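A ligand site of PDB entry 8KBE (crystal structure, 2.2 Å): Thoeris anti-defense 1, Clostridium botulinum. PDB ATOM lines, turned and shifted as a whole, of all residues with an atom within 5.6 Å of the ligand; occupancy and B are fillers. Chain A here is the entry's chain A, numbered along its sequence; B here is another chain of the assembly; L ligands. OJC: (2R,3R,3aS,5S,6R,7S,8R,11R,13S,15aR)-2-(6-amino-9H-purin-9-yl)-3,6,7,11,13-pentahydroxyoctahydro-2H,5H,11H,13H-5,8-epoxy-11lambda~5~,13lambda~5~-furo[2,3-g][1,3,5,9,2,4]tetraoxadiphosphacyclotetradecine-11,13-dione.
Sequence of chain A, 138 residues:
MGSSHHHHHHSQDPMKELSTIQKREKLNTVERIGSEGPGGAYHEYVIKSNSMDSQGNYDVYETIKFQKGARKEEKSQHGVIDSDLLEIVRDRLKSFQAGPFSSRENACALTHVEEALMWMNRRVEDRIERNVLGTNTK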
ATOM      1  N   PRO A  38      -6.492 -36.184  -9.740  1.00  0.00           N
ATOM      2  CA  PRO A  38      -5.978 -35.326  -8.661  1.00  0.00           C
ATOM      3  C   PRO A  38      -7.068 -34.955  -7.663  1.00  0.00           C
ATOM      4  O   PRO A  38      -8.211 -34.681  -8.023  1.00  0.00           O
ATOM      5  CB  PRO A  38      -5.472 -34.088  -9.418  1.00  0.00           C
ATOM      6  CG  PRO A  38      -5.199 -34.562 -10.803  1.00  0.00           C
ATOM      7  CD  PRO A  38      -6.172 -35.671 -11.078  1.00  0.00           C
ATOM      8  N   GLY A  39      -6.701 -34.983  -6.380  1.00  0.00           N
ATOM      9  CA  GLY A  39      -7.639 -34.670  -5.321  1.00  0.00           C
ATOM     10  C   GLY A  39      -8.727 -35.693  -5.083  1.00  0.00           C
ATOM     11  O   GLY A  39      -9.586 -35.465  -4.224  1.00  0.00           O
ATOM     12  N   GLY A  40      -8.732 -36.796  -5.818  1.00  0.00           N
ATOM     13  CA  GLY A  40      -9.817 -37.757  -5.699  1.00  0.00           C
ATOM     14  C   GLY A  40     -11.062 -37.414  -6.490  1.00  0.00           C
ATOM     15  O   GLY A  40     -12.127 -37.988  -6.217  1.00  0.00           O
ATOM     16  N   HIS A  43     -12.624 -35.572 -13.670  1.00  0.00           N
ATOM     17  CA  HIS A  43     -12.340 -34.370 -14.439  1.00  0.00           C
ATOM     18  C   HIS A  43     -12.991 -34.373 -15.818  1.00  0.00           C
ATOM     19  O   HIS A  43     -12.643 -33.528 -16.654  1.00  0.00           O
ATOM     20  CB  HIS A  43     -10.823 -34.156 -14.562  1.00  0.00           C
ATOM     21  CG  HIS A  43     -10.141 -33.910 -13.259  1.00  0.00           C
ATOM     22  ND1 HIS A  43     -10.042 -34.867 -12.270  1.00  0.00           N
ATOM     23  CD2 HIS A  43      -9.517 -32.813 -12.767  1.00  0.00           C
ATOM     24  CE1 HIS A  43      -9.392 -34.379 -11.233  1.00  0.00           C
ATOM     25  NE2 HIS A  43      -9.062 -33.127 -11.506  1.00  0.00           N
ATOM     26  N   PHE A  66     -12.479 -30.752 -16.886  1.00  0.00           N
ATOM     27  CA  PHE A  66     -11.977 -29.835 -15.878  1.00  0.00           C
ATOM     28  C   PHE A  66     -10.462 -29.728 -15.936  1.00  0.00           C
ATOM     29  O   PHE A  66      -9.772 -30.690 -16.282  1.00  0.00           O
ATOM     30  CB  PHE A  66     -12.402 -30.259 -14.468  1.00  0.00           C
ATOM     31  CG  PHE A  66     -13.837 -29.963 -14.162  1.00  0.00           C
ATOM     32  CD1 PHE A  66     -14.812 -30.880 -14.479  1.00  0.00           C
ATOM     33  CD2 PHE A  66     -14.200 -28.764 -13.566  1.00  0.00           C
ATOM     34  CE1 PHE A  66     -16.143 -30.620 -14.223  1.00  0.00           C
ATOM     35  CE2 PHE A  66     -15.534 -28.492 -13.298  1.00  0.00           C
ATOM     36  CZ  PHE A  66     -16.506 -29.420 -13.627  1.00  0.00           C
ATOM     37  N   GLN A  67      -9.968 -28.536 -15.619  1.00  0.00           N
ATOM     38  CA  GLN A  67      -8.577 -28.361 -15.267  1.00  0.00           C
ATOM     39  C   GLN A  67      -8.129 -29.501 -14.368  1.00  0.00           C
ATOM     40  O   GLN A  67      -8.615 -29.638 -13.244  1.00  0.00           O
ATOM     41  CB  GLN A  67      -8.398 -27.019 -14.543  1.00  0.00           C
ATOM     42  CG  GLN A  67      -6.985 -26.737 -14.082  1.00  0.00           C
ATOM     43  CD  GLN A  67      -6.075 -26.385 -15.237  1.00  0.00           C
ATOM     44  OE1 GLN A  67      -6.486 -25.728 -16.193  1.00  0.00           O
ATOM     45  NE2 GLN A  67      -4.819 -26.816 -15.144  1.00  0.00           N
ATOM     46  N   LYS A  68      -7.200 -30.321 -14.868  1.00  0.00           N
ATOM     47  CA  LYS A  68      -6.828 -31.580 -14.239  1.00  0.00           C
ATOM     48  C   LYS A  68      -5.381 -31.459 -13.790  1.00  0.00           C
ATOM     49  O   LYS A  68      -4.470 -31.420 -14.625  1.00  0.00           O
ATOM     50  CB  LYS A  68      -7.013 -32.745 -15.206  1.00  0.00           C
ATOM     51  CG  LYS A  68      -6.774 -34.134 -14.645  1.00  0.00           C
ATOM     52  CD  LYS A  68      -7.243 -35.201 -15.644  1.00  0.00           C
ATOM     53  CE  LYS A  68      -6.974 -36.612 -15.136  1.00  0.00           C
ATOM     54  NZ  LYS A  68      -7.399 -37.656 -16.120  1.00  0.00           N
ATOM     55  N   GLY A  69      -5.164 -31.422 -12.482  1.00  0.00           N
ATOM     56  CA  GLY A  69      -3.839 -31.118 -11.977  1.00  0.00           C
ATOM     57  C   GLY A  69      -3.685 -29.632 -11.821  1.00  0.00           C
ATOM     58  O   GLY A  69      -4.111 -28.862 -12.686  1.00  0.00           O
ATOM     59  N   ALA A  70      -3.075 -29.191 -10.715  1.00  0.00           N
ATOM     60  CA  ALA A  70      -3.031 -27.771 -10.400  1.00  0.00           C
ATOM     61  C   ALA A  70      -2.245 -26.995 -11.455  1.00  0.00           C
ATOM     62  O   ALA A  70      -1.364 -27.542 -12.139  1.00  0.00           O
ATOM     63  CB  ALA A  70      -2.421 -27.585  -9.016  1.00  0.00           C
ATOM     64  N   ARG A  71      -2.579 -25.706 -11.595  1.00  0.00           N
ATOM     65  CA  ARG A  71      -2.170 -24.964 -12.786  1.00  0.00           C
ATOM     66  C   ARG A  71      -0.669 -24.712 -12.860  1.00  0.00           C
ATOM     67  O   ARG A  71      -0.132 -24.533 -13.960  1.00  0.00           O
ATOM     68  CB  ARG A  71      -2.912 -23.623 -12.848  1.00  0.00           C
ATOM     69  CG  ARG A  71      -2.380 -22.555 -11.915  1.00  0.00           C
ATOM     70  CD  ARG A  71      -3.343 -21.381 -11.819  1.00  0.00           C
ATOM     71  NE  ARG A  71      -4.549 -21.702 -11.066  1.00  0.00           N
ATOM     72  CZ  ARG A  71      -5.480 -20.811 -10.704  1.00  0.00           C
ATOM     73  NH1 ARG A  71      -5.345 -19.534 -11.043  1.00  0.00           N
ATOM     74  NH2 ARG A  71      -6.550 -21.197 -10.012  1.00  0.00           N
ATOM     75  N   LYS A  72       0.039 -24.711 -11.737  1.00  0.00           N
ATOM     76  CA  LYS A  72       1.477 -24.453 -11.777  1.00  0.00           C
ATOM     77  C   LYS A  72       2.308 -25.732 -11.866  1.00  0.00           C
ATOM     78  O   LYS A  72       3.513 -25.645 -12.095  1.00  0.00           O
ATOM     79  CB  LYS A  72       1.921 -23.670 -10.544  1.00  0.00           C
ATOM     80  CG  LYS A  72       1.423 -22.234 -10.430  1.00  0.00           C
ATOM     81  CD  LYS A  72       1.811 -21.674  -9.059  1.00  0.00           C
ATOM     82  CE  LYS A  72       1.270 -20.271  -8.833  1.00  0.00           C
ATOM     83  NZ  LYS A  72       1.710 -19.717  -7.524  1.00  0.00           N
ATOM     84  N   ILE A  81     -13.017 -24.638 -14.630  1.00  0.00           N
ATOM     85  CA  ILE A  81     -13.037 -24.787 -13.191  1.00  0.00           C
ATOM     86  C   ILE A  81     -14.466 -24.587 -12.663  1.00  0.00           C
ATOM     87  O   ILE A  81     -15.309 -23.958 -13.296  1.00  0.00           O
ATOM     88  CB  ILE A  81     -12.040 -23.825 -12.497  1.00  0.00           C
ATOM     89  CG1 ILE A  81     -11.614 -24.392 -11.151  1.00  0.00           C
ATOM     90  CG2 ILE A  81     -12.639 -22.437 -12.357  1.00  0.00           C
ATOM     91  CD1 ILE A  81     -10.847 -25.680 -11.259  1.00  0.00           C
ATOM     92  N   ASP A  82     -14.728 -25.156 -11.485  1.00  0.00           N
ATOM     93  CA  ASP A  82     -16.090 -25.302 -10.993  1.00  0.00           C
ATOM     94  C   ASP A  82     -16.797 -23.953 -10.855  1.00  0.00           C
ATOM     95  O   ASP A  82     -17.992 -23.827 -11.142  1.00  0.00           O
ATOM     96  CB  ASP A  82     -16.062 -26.065  -9.679  1.00  0.00           C
ATOM     97  CG  ASP A  82     -15.296 -27.384  -9.797  1.00  0.00           C
ATOM     98  OD1 ASP A  82     -14.049 -27.354  -9.850  1.00  0.00           O
ATOM     99  OD2 ASP A  82     -15.946 -28.439  -9.830  1.00  0.00           O
ATOM    100  N   MET A 120     -16.089 -20.599  -2.454  1.00  0.00           N
ATOM    101  CA  MET A 120     -15.034 -21.007  -3.375  1.00  0.00           C
ATOM    102  C   MET A 120     -13.956 -19.941  -3.492  1.00  0.00           C
ATOM    103  O   MET A 120     -12.761 -20.235  -3.505  1.00  0.00           O
ATOM    104  CB  MET A 120     -15.638 -21.316  -4.751  1.00  0.00           C
ATOM    105  CG  MET A 120     -16.509 -22.568  -4.754  1.00  0.00           C
ATOM    106  SD  MET A 120     -17.377 -22.724  -6.318  1.00  0.00           S
ATOM    107  CE  MET A 120     -17.097 -24.452  -6.681  1.00  0.00           C
ATOM    108  N   ARG A 123     -11.852 -19.958  -0.427  1.00  0.00           N
ATOM    109  CA  ARG A 123     -10.791 -20.952  -0.582  1.00  0.00           C
ATOM    110  C   ARG A 123      -9.648 -20.410  -1.440  1.00  0.00           C
ATOM    111  O   ARG A 123      -8.462 -20.571  -1.096  1.00  0.00           O
ATOM    112  CB  ARG A 123     -11.365 -22.233  -1.199  1.00  0.00           C
ATOM    113  CG  ARG A 123     -10.336 -23.344  -1.363  1.00  0.00           C
ATOM    114  CD  ARG A 123     -10.873 -24.553  -2.133  1.00  0.00           C
ATOM    115  NE  ARG A 123      -9.808 -25.526  -2.407  1.00  0.00           N
ATOM    116  CZ  ARG A 123      -9.087 -25.562  -3.523  1.00  0.00           C
ATOM    117  NH1 ARG A 123      -9.324 -24.685  -4.480  1.00  0.00           N
ATOM    118  NH2 ARG A 123      -8.141 -26.471  -3.687  1.00  0.00           N
ATOM    119  N   ARG A 127      -5.749 -19.805  -0.258  1.00  0.00           N
ATOM    120  CA  ARG A 127      -4.609 -20.484  -0.869  1.00  0.00           C
ATOM    121  C   ARG A 127      -3.613 -19.489  -1.448  1.00  0.00           C
ATOM    122  O   ARG A 127      -2.408 -19.777  -1.496  1.00  0.00           O
ATOM    123  CB  ARG A 127      -5.074 -21.474  -1.934  1.00  0.00           C
ATOM    124  CG  ARG A 127      -5.944 -22.602  -1.404  1.00  0.00           C
ATOM    125  CD  ARG A 127      -6.306 -23.595  -2.486  1.00  0.00           C
ATOM    126  NE  ARG A 127      -5.121 -24.237  -3.029  1.00  0.00           N
ATOM    127  CZ  ARG A 127      -4.518 -25.283  -2.476  1.00  0.00           C
ATOM    128  NH1 ARG A 127      -4.994 -25.801  -1.346  1.00  0.00           N
ATOM    129  NH2 ARG A 127      -3.442 -25.801  -3.042  1.00  0.00           N
ATOM    130  N   VAL A 132      -0.166 -21.321  -1.828  1.00  0.00           N
ATOM    131  CA  VAL A 132      -0.220 -22.676  -2.385  1.00  0.00           C
ATOM    132  C   VAL A 132      -1.144 -22.771  -3.586  1.00  0.00           C
ATOM    133  O   VAL A 132      -1.365 -23.863  -4.113  1.00  0.00           O
ATOM    134  CB  VAL A 132      -0.616 -23.718  -1.317  1.00  0.00           C
ATOM    135  CG1 VAL A 132       0.386 -23.706  -0.177  1.00  0.00           C
ATOM    136  CG2 VAL A 132      -2.030 -23.462  -0.816  1.00  0.00           C
ATOM    137  N   LEU A 133      -1.701 -21.656  -4.060  1.00  0.00           N
ATOM    138  CA  LEU A 133      -2.631 -21.713  -5.184  1.00  0.00           C
ATOM    139  C   LEU A 133      -1.936 -22.245  -6.429  1.00  0.00           C
ATOM    140  O   LEU A 133      -0.854 -21.774  -6.794  1.00  0.00           O
ATOM    141  CB  LEU A 133      -3.219 -20.331  -5.475  1.00  0.00           C
ATOM    142  CG  LEU A 133      -4.303 -20.353  -6.563  1.00  0.00           C
ATOM    143  CD1 LEU A 133      -5.557 -21.062  -6.037  1.00  0.00           C
ATOM    144  CD2 LEU A 133      -4.623 -18.961  -7.051  1.00  0.00           C
ATOM    145  N   GLY A 134      -2.557 -23.211  -7.083  1.00  0.00           N
ATOM    146  CA  GLY A 134      -1.972 -23.817  -8.254  1.00  0.00           C
ATOM    147  C   GLY A 134      -0.981 -24.916  -7.976  1.00  0.00           C
ATOM    148  O   GLY A 134      -0.266 -25.324  -8.898  1.00  0.00           O
ATOM    149  N   THR A 135      -0.911 -25.417  -6.742  1.00  0.00           N
ATOM    150  CA  THR A 135      -0.059 -26.542  -6.379  1.00  0.00           C
ATOM    151  C   THR A 135      -0.881 -27.569  -5.610  1.00  0.00           C
ATOM    152  O   THR A 135      -1.932 -27.252  -5.054  1.00  0.00           O
ATOM    153  CB  THR A 135       1.145 -26.103  -5.529  1.00  0.00           C
ATOM    154  OG1 THR A 135       0.730 -25.959  -4.165  1.00  0.00           O
ATOM    155  CG2 THR A 135       1.711 -24.786  -6.030  1.00  0.00           C
ATOM    156  N   ASN A 136      -0.385 -28.810  -5.594  1.00  0.00           N
ATOM    157  CA  ASN A 136      -1.049 -29.905  -4.885  1.00  0.00           C
ATOM    158  C   ASN A 136      -0.615 -29.932  -3.424  1.00  0.00           C
ATOM    159  O   ASN A 136       0.182 -30.763  -2.988  1.00  0.00           O
ATOM    160  CB  ASN A 136      -0.783 -31.237  -5.595  1.00  0.00           C
ATOM    161  CG  ASN A 136      -1.289 -31.233  -7.028  1.00  0.00           C
ATOM    162  OD1 ASN A 136      -0.595 -30.786  -7.942  1.00  0.00           O
ATOM    163  ND2 ASN A 136      -2.512 -31.720  -7.230  1.00  0.00           N
ATOM    164  N   THR A 137      -1.162 -28.997  -2.652  1.00  0.00           N
ATOM    165  CA  THR A 137      -0.865 -28.845  -1.235  1.00  0.00           C
ATOM    166  C   THR A 137      -2.163 -28.594  -0.479  1.00  0.00           C
ATOM    167  O   THR A 137      -3.074 -27.952  -1.012  1.00  0.00           O
ATOM    168  CB  THR A 137       0.112 -27.698  -0.973  1.00  0.00           C
ATOM    169  OG1 THR A 137       1.212 -27.778  -1.900  1.00  0.00           O
ATOM    170  CG2 THR A 137       0.645 -27.747   0.472  1.00  0.00           C
ATOM    171  N   LEU B  27      -8.568 -18.345 -13.408  1.00  0.00           N
ATOM    172  CA  LEU B  27      -8.111 -19.214 -14.489  1.00  0.00           C
ATOM    173  C   LEU B  27      -8.714 -18.813 -15.822  1.00  0.00           C
ATOM    174  O   LEU B  27      -8.014 -18.691 -16.834  1.00  0.00           O
ATOM    175  CB  LEU B  27      -8.469 -20.675 -14.216  1.00  0.00           C
ATOM    176  CG  LEU B  27      -7.558 -21.662 -13.523  1.00  0.00           C
ATOM    177  CD1 LEU B  27      -8.215 -23.030 -13.639  1.00  0.00           C
ATOM    178  CD2 LEU B  27      -6.223 -21.671 -14.218  1.00  0.00           C
ATOM    179  N   ARG B  92     -18.164 -32.930  -7.852  1.00  0.00           N
ATOM    180  CA  ARG B  92     -16.750 -32.630  -7.691  1.00  0.00           C
ATOM    181  C   ARG B  92     -16.437 -32.224  -6.248  1.00  0.00           C
ATOM    182  O   ARG B  92     -15.392 -32.606  -5.702  1.00  0.00           O
ATOM    183  CB  ARG B  92     -16.311 -31.574  -8.711  1.00  0.00           C
ATOM    184  CG  ARG B  92     -15.996 -32.257 -10.026  1.00  0.00           C
ATOM    185  CD  ARG B  92     -15.322 -31.415 -11.071  1.00  0.00           C
ATOM    186  NE  ARG B  92     -14.351 -30.435 -10.603  1.00  0.00           N
ATOM    187  CZ  ARG B  92     -13.031 -30.575 -10.673  1.00  0.00           C
ATOM    188  NH1 ARG B  92     -12.503 -31.699 -11.171  1.00  0.00           N
ATOM    189  NH2 ARG B  92     -12.230 -29.612 -10.237  1.00  0.00           N
ATOM    190  N   LEU B  93     -17.304 -31.418  -5.633  1.00  0.00           N
ATOM    191  CA  LEU B  93     -17.082 -31.018  -4.252  1.00  0.00           C
ATOM    192  C   LEU B  93     -17.169 -32.216  -3.311  1.00  0.00           C
ATOM    193  O   LEU B  93     -16.350 -32.347  -2.391  1.00  0.00           O
ATOM    194  CB  LEU B  93     -18.065 -29.919  -3.871  1.00  0.00           C
ATOM    195  CG  LEU B  93     -17.768 -28.544  -4.484  1.00  0.00           C
ATOM    196  CD1 LEU B  93     -18.772 -27.488  -4.042  1.00  0.00           C
ATOM    197  CD2 LEU B  93     -16.384 -28.105  -4.055  1.00  0.00           C
ATOM    198  N   PHE B  96     -13.783 -34.064  -3.786  1.00  0.00           N
ATOM    199  CA  PHE B  96     -12.708 -33.355  -3.101  1.00  0.00           C
ATOM    200  C   PHE B  96     -12.826 -33.477  -1.593  1.00  0.00           C
ATOM    201  O   PHE B  96     -11.802 -33.536  -0.899  1.00  0.00           O
ATOM    202  CB  PHE B  96     -12.695 -31.883  -3.512  1.00  0.00           C
ATOM    203  CG  PHE B  96     -12.116 -31.621  -4.873  1.00  0.00           C
ATOM    204  CD1 PHE B  96     -10.989 -32.313  -5.308  1.00  0.00           C
ATOM    205  CD2 PHE B  96     -12.684 -30.687  -5.727  1.00  0.00           C
ATOM    206  CE1 PHE B  96     -10.454 -32.075  -6.568  1.00  0.00           C
ATOM    207  CE2 PHE B  96     -12.155 -30.437  -6.984  1.00  0.00           C
ATOM    208  CZ  PHE B  96     -11.037 -31.137  -7.406  1.00  0.00           C
ATOM    209  N   PHE B 101      -7.556 -33.450   0.226  1.00  0.00           N
ATOM    210  CA  PHE B 101      -7.465 -31.992   0.235  1.00  0.00           C
ATOM    211  C   PHE B 101      -8.802 -31.353   0.611  1.00  0.00           C
ATOM    212  O   PHE B 101      -9.217 -30.360   0.009  1.00  0.00           O
ATOM    213  CB  PHE B 101      -6.988 -31.482  -1.120  1.00  0.00           C
ATOM    214  CG  PHE B 101      -5.582 -31.866  -1.447  1.00  0.00           C
ATOM    215  CD1 PHE B 101      -4.511 -31.224  -0.846  1.00  0.00           C
ATOM    216  CD2 PHE B 101      -5.313 -32.886  -2.350  1.00  0.00           C
ATOM    217  CE1 PHE B 101      -3.209 -31.583  -1.144  1.00  0.00           C
ATOM    218  CE2 PHE B 101      -4.015 -33.245  -2.658  1.00  0.00           C
ATOM    219  CZ  PHE B 101      -2.960 -32.589  -2.050  1.00  0.00           C
ATOM    220  N   SER B 102      -9.463 -31.902   1.618  1.00  0.00           N
ATOM    221  CA  SER B 102     -10.741 -31.362   2.068  1.00  0.00           C
ATOM    222  C   SER B 102     -10.555 -29.995   2.736  1.00  0.00           C
ATOM    223  O   SER B 102      -9.443 -29.571   3.033  1.00  0.00           O
ATOM    224  CB  SER B 102     -11.412 -32.343   3.036  1.00  0.00           C
ATOM    225  OG  SER B 102     -10.641 -32.453   4.221  1.00  0.00           O
ATOM    226  N   SER B 103     -11.673 -29.311   2.965  1.00  0.00           N
ATOM    227  CA  SER B 103     -11.631 -28.008   3.612  1.00  0.00           C
ATOM    228  C   SER B 103     -13.023 -27.625   4.093  1.00  0.00           C
ATOM    229  O   SER B 103     -14.038 -28.109   3.568  1.00  0.00           O
ATOM    230  CB  SER B 103     -11.086 -26.937   2.659  1.00  0.00           C
ATOM    231  OG  SER B 103     -11.912 -26.803   1.517  1.00  0.00           O
ATOM    232  N   ASN B 106     -14.744 -25.853   1.184  1.00  0.00           N
ATOM    233  CA  ASN B 106     -15.422 -26.843   0.338  1.00  0.00           C
ATOM    234  C   ASN B 106     -16.731 -27.297   0.960  1.00  0.00           C
ATOM    235  O   ASN B 106     -17.733 -27.429   0.247  1.00  0.00           O
ATOM    236  CB  ASN B 106     -14.510 -28.058   0.102  1.00  0.00           C
ATOM    237  CG  ASN B 106     -13.462 -27.810  -0.967  1.00  0.00           C
ATOM    238  OD1 ASN B 106     -13.489 -26.815  -1.672  1.00  0.00           O
ATOM    239  ND2 ASN B 106     -12.517 -28.746  -1.088  1.00  0.00           N
HETATM  240  N   OJC L   1     -11.521 -26.993  -6.336  1.00  0.00           N
HETATM  241  C   OJC L   1     -10.430 -27.427  -6.971  1.00  0.00           C
HETATM  242  O   OJC L   1      -6.542 -29.066  -4.504  1.00  0.00           O
HETATM  243  C1  OJC L   1     -11.724 -27.361  -5.041  1.00  0.00           C
HETATM  244  C2  OJC L   1     -10.735 -28.179  -4.452  1.00  0.00           C
HETATM  245  C3  OJC L   1      -9.662 -28.558  -5.230  1.00  0.00           C
HETATM  246  C10 OJC L   1      -7.344 -26.898 -10.078  1.00  0.00           C
HETATM  247  C11 OJC L   1      -7.111 -28.369 -10.295  1.00  0.00           C
HETATM  248  C12 OJC L   1      -8.218 -29.307  -9.814  1.00  0.00           C
HETATM  249  C13 OJC L   1      -7.444 -30.565  -9.400  1.00  0.00           C
HETATM  250  C14 OJC L   1      -6.018 -30.075  -9.126  1.00  0.00           C
HETATM  251  C4  OJC L   1      -9.509 -29.395  -3.215  1.00  0.00           C
HETATM  252  C5  OJC L   1      -7.591 -30.017  -4.675  1.00  0.00           C
HETATM  253  C6  OJC L   1      -7.343 -30.689  -6.030  1.00  0.00           C
HETATM  254  C7  OJC L   1      -6.544 -29.624  -6.769  1.00  0.00           C
HETATM  255  C8  OJC L   1      -5.665 -29.095  -5.646  1.00  0.00           C
HETATM  256  C9  OJC L   1      -5.125 -27.703  -5.914  1.00  0.00           C
HETATM  257  N1  OJC L   1      -9.447 -28.193  -6.519  1.00  0.00           N
HETATM  258  N2  OJC L   1      -8.865 -29.339  -4.419  1.00  0.00           N
HETATM  259  N3  OJC L   1     -10.642 -28.733  -3.183  1.00  0.00           N
HETATM  260  N4  OJC L   1     -12.806 -26.929  -4.409  1.00  0.00           N
HETATM  261  O1  OJC L   1      -6.240 -26.861  -6.273  1.00  0.00           O
HETATM  262  O10 OJC L   1      -7.447 -31.548 -10.436  1.00  0.00           O
HETATM  263  O11 OJC L   1      -9.193 -29.560 -10.815  1.00  0.00           O
HETATM  264  O12 OJC L   1      -6.546 -31.827  -5.860  1.00  0.00           O
HETATM  265  O2  OJC L   1      -7.133 -24.574  -5.915  1.00  0.00           O
HETATM  266  O3  OJC L   1      -4.597 -24.934  -6.048  1.00  0.00           O
HETATM  267  O4  OJC L   1      -6.179 -24.872  -8.048  1.00  0.00           O
HETATM  268  O5  OJC L   1      -6.993 -23.923 -10.146  1.00  0.00           O
HETATM  269  O6  OJC L   1      -4.524 -24.332  -9.901  1.00  0.00           O
HETATM  270  O7  OJC L   1      -6.092 -26.246 -10.283  1.00  0.00           O
HETATM  271  O8  OJC L   1      -5.968 -28.710  -9.486  1.00  0.00           O
HETATM  272  O9  OJC L   1      -5.705 -30.187  -7.758  1.00  0.00           O
HETATM  273  P   OJC L   1      -5.963 -25.298  -6.505  1.00  0.00           P
HETATM  274  P1  OJC L   1      -5.908 -24.808  -9.636  1.00  0.00           P
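Pro 38 touches the ligand (CB to O10, 3.4 Å).
Lys 68 touches the ligand (CA to O10, 3.9 Å).
CD1 of Ile 81 touches C10 of the ligand, 3.9 Å away.
O of Val 132 touches O3 of the ligand (3.9 Å).
C of Leu 133 touches O3 of the ligand, 3.8 Å away.
Thr 135 touches the ligand (O to C9, 3.3 Å).
Asn 136 touches the ligand.
CD1 of Leu 27 of chain B touches O5 of the ligand (3.8 Å).
Leu 93 of chain B touches the ligand (CD2 to N4, 3.8 Å).
Phe 96 of chain B touches the ligand (CD2 to C2, 3.4 Å).
Phe 101 of chain B touches the ligand.
Hydrophobic or aromatic side chains that line the ligand: Pro 38, His 43, Ala 70, Ile 81, Leu 133, Leu 27 of chain B, Leu 93 of chain B, Phe 96 of chain B and Phe 101 of chain B.
The backbone carbonyl oxygen of Thr 135 sits at hydrogen-bond distance from the guanidinium group of Arg 127.
The backbone NH of Asn 106 of chain B lies within hydrogen-bond range of the side-chain hydroxyl of Ser 103 of chain B (3.0 Å).
NE of Arg 92 of chain B lies within salt-bridge range of OD2 of Asp 82, 2.7 Å away.
N of Val 132 sits at hydrogen-bond distance from O of Arg 127, 2.7 Å away.
NH1 of Arg 127 sits at hydrogen-bond distance from O of Thr 137 (2.9 Å).
N of Leu 133 is in hydrogen-bond range of O of Arg 127.
O of Leu 133 lies close to NZ of Lys 72, 3.4 Å away.
OG1 of Thr 137 sits at hydrogen-bond distance from OG1 of Thr 135 (2.9 Å).
N of Gly 69 sits at hydrogen-bond distance from O10 of the ligand (3.1 Å).
ND2 of Asn 106 of chain B is in hydrogen-bond range of N3 of the ligand, 2.8 Å away.
NH2 of Arg 71 lies within salt-bridge range of O5 of the ligand (2.8 Å).
N of Ala 70 sits at hydrogen-bond distance from O8 of the ligand (3.2 Å).
An oxygen (O3) of the ligand is in hydrogen-bond range of the backbone NH (N) of Gly 134, 2.9 Å away.
NE of Arg 127 lies within salt-bridge range of O3 of the ligand (3.1 Å).
O10 of the ligand sits at hydrogen-bond distance from NE2 of His 43.
N of Gly 39 lies close to O12 of the ligand, 3.2 Å away.
O2 of the ligand is in salt-bridge range of NH1 of Arg 123 (2.6 Å).
An oxygen (O11) of the ligand is in hydrogen-bond range of the backbone carbonyl oxygen (O) of Gln 67.
The backbone NH of Arg 71 lies within hydrogen-bond range of an oxygen (O6) of the ligand, 2.9 Å away.
The guanidinium group of Arg 92 of chain B is in hydrogen-bond range of an oxygen (O11) of the ligand (3.1 Å).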
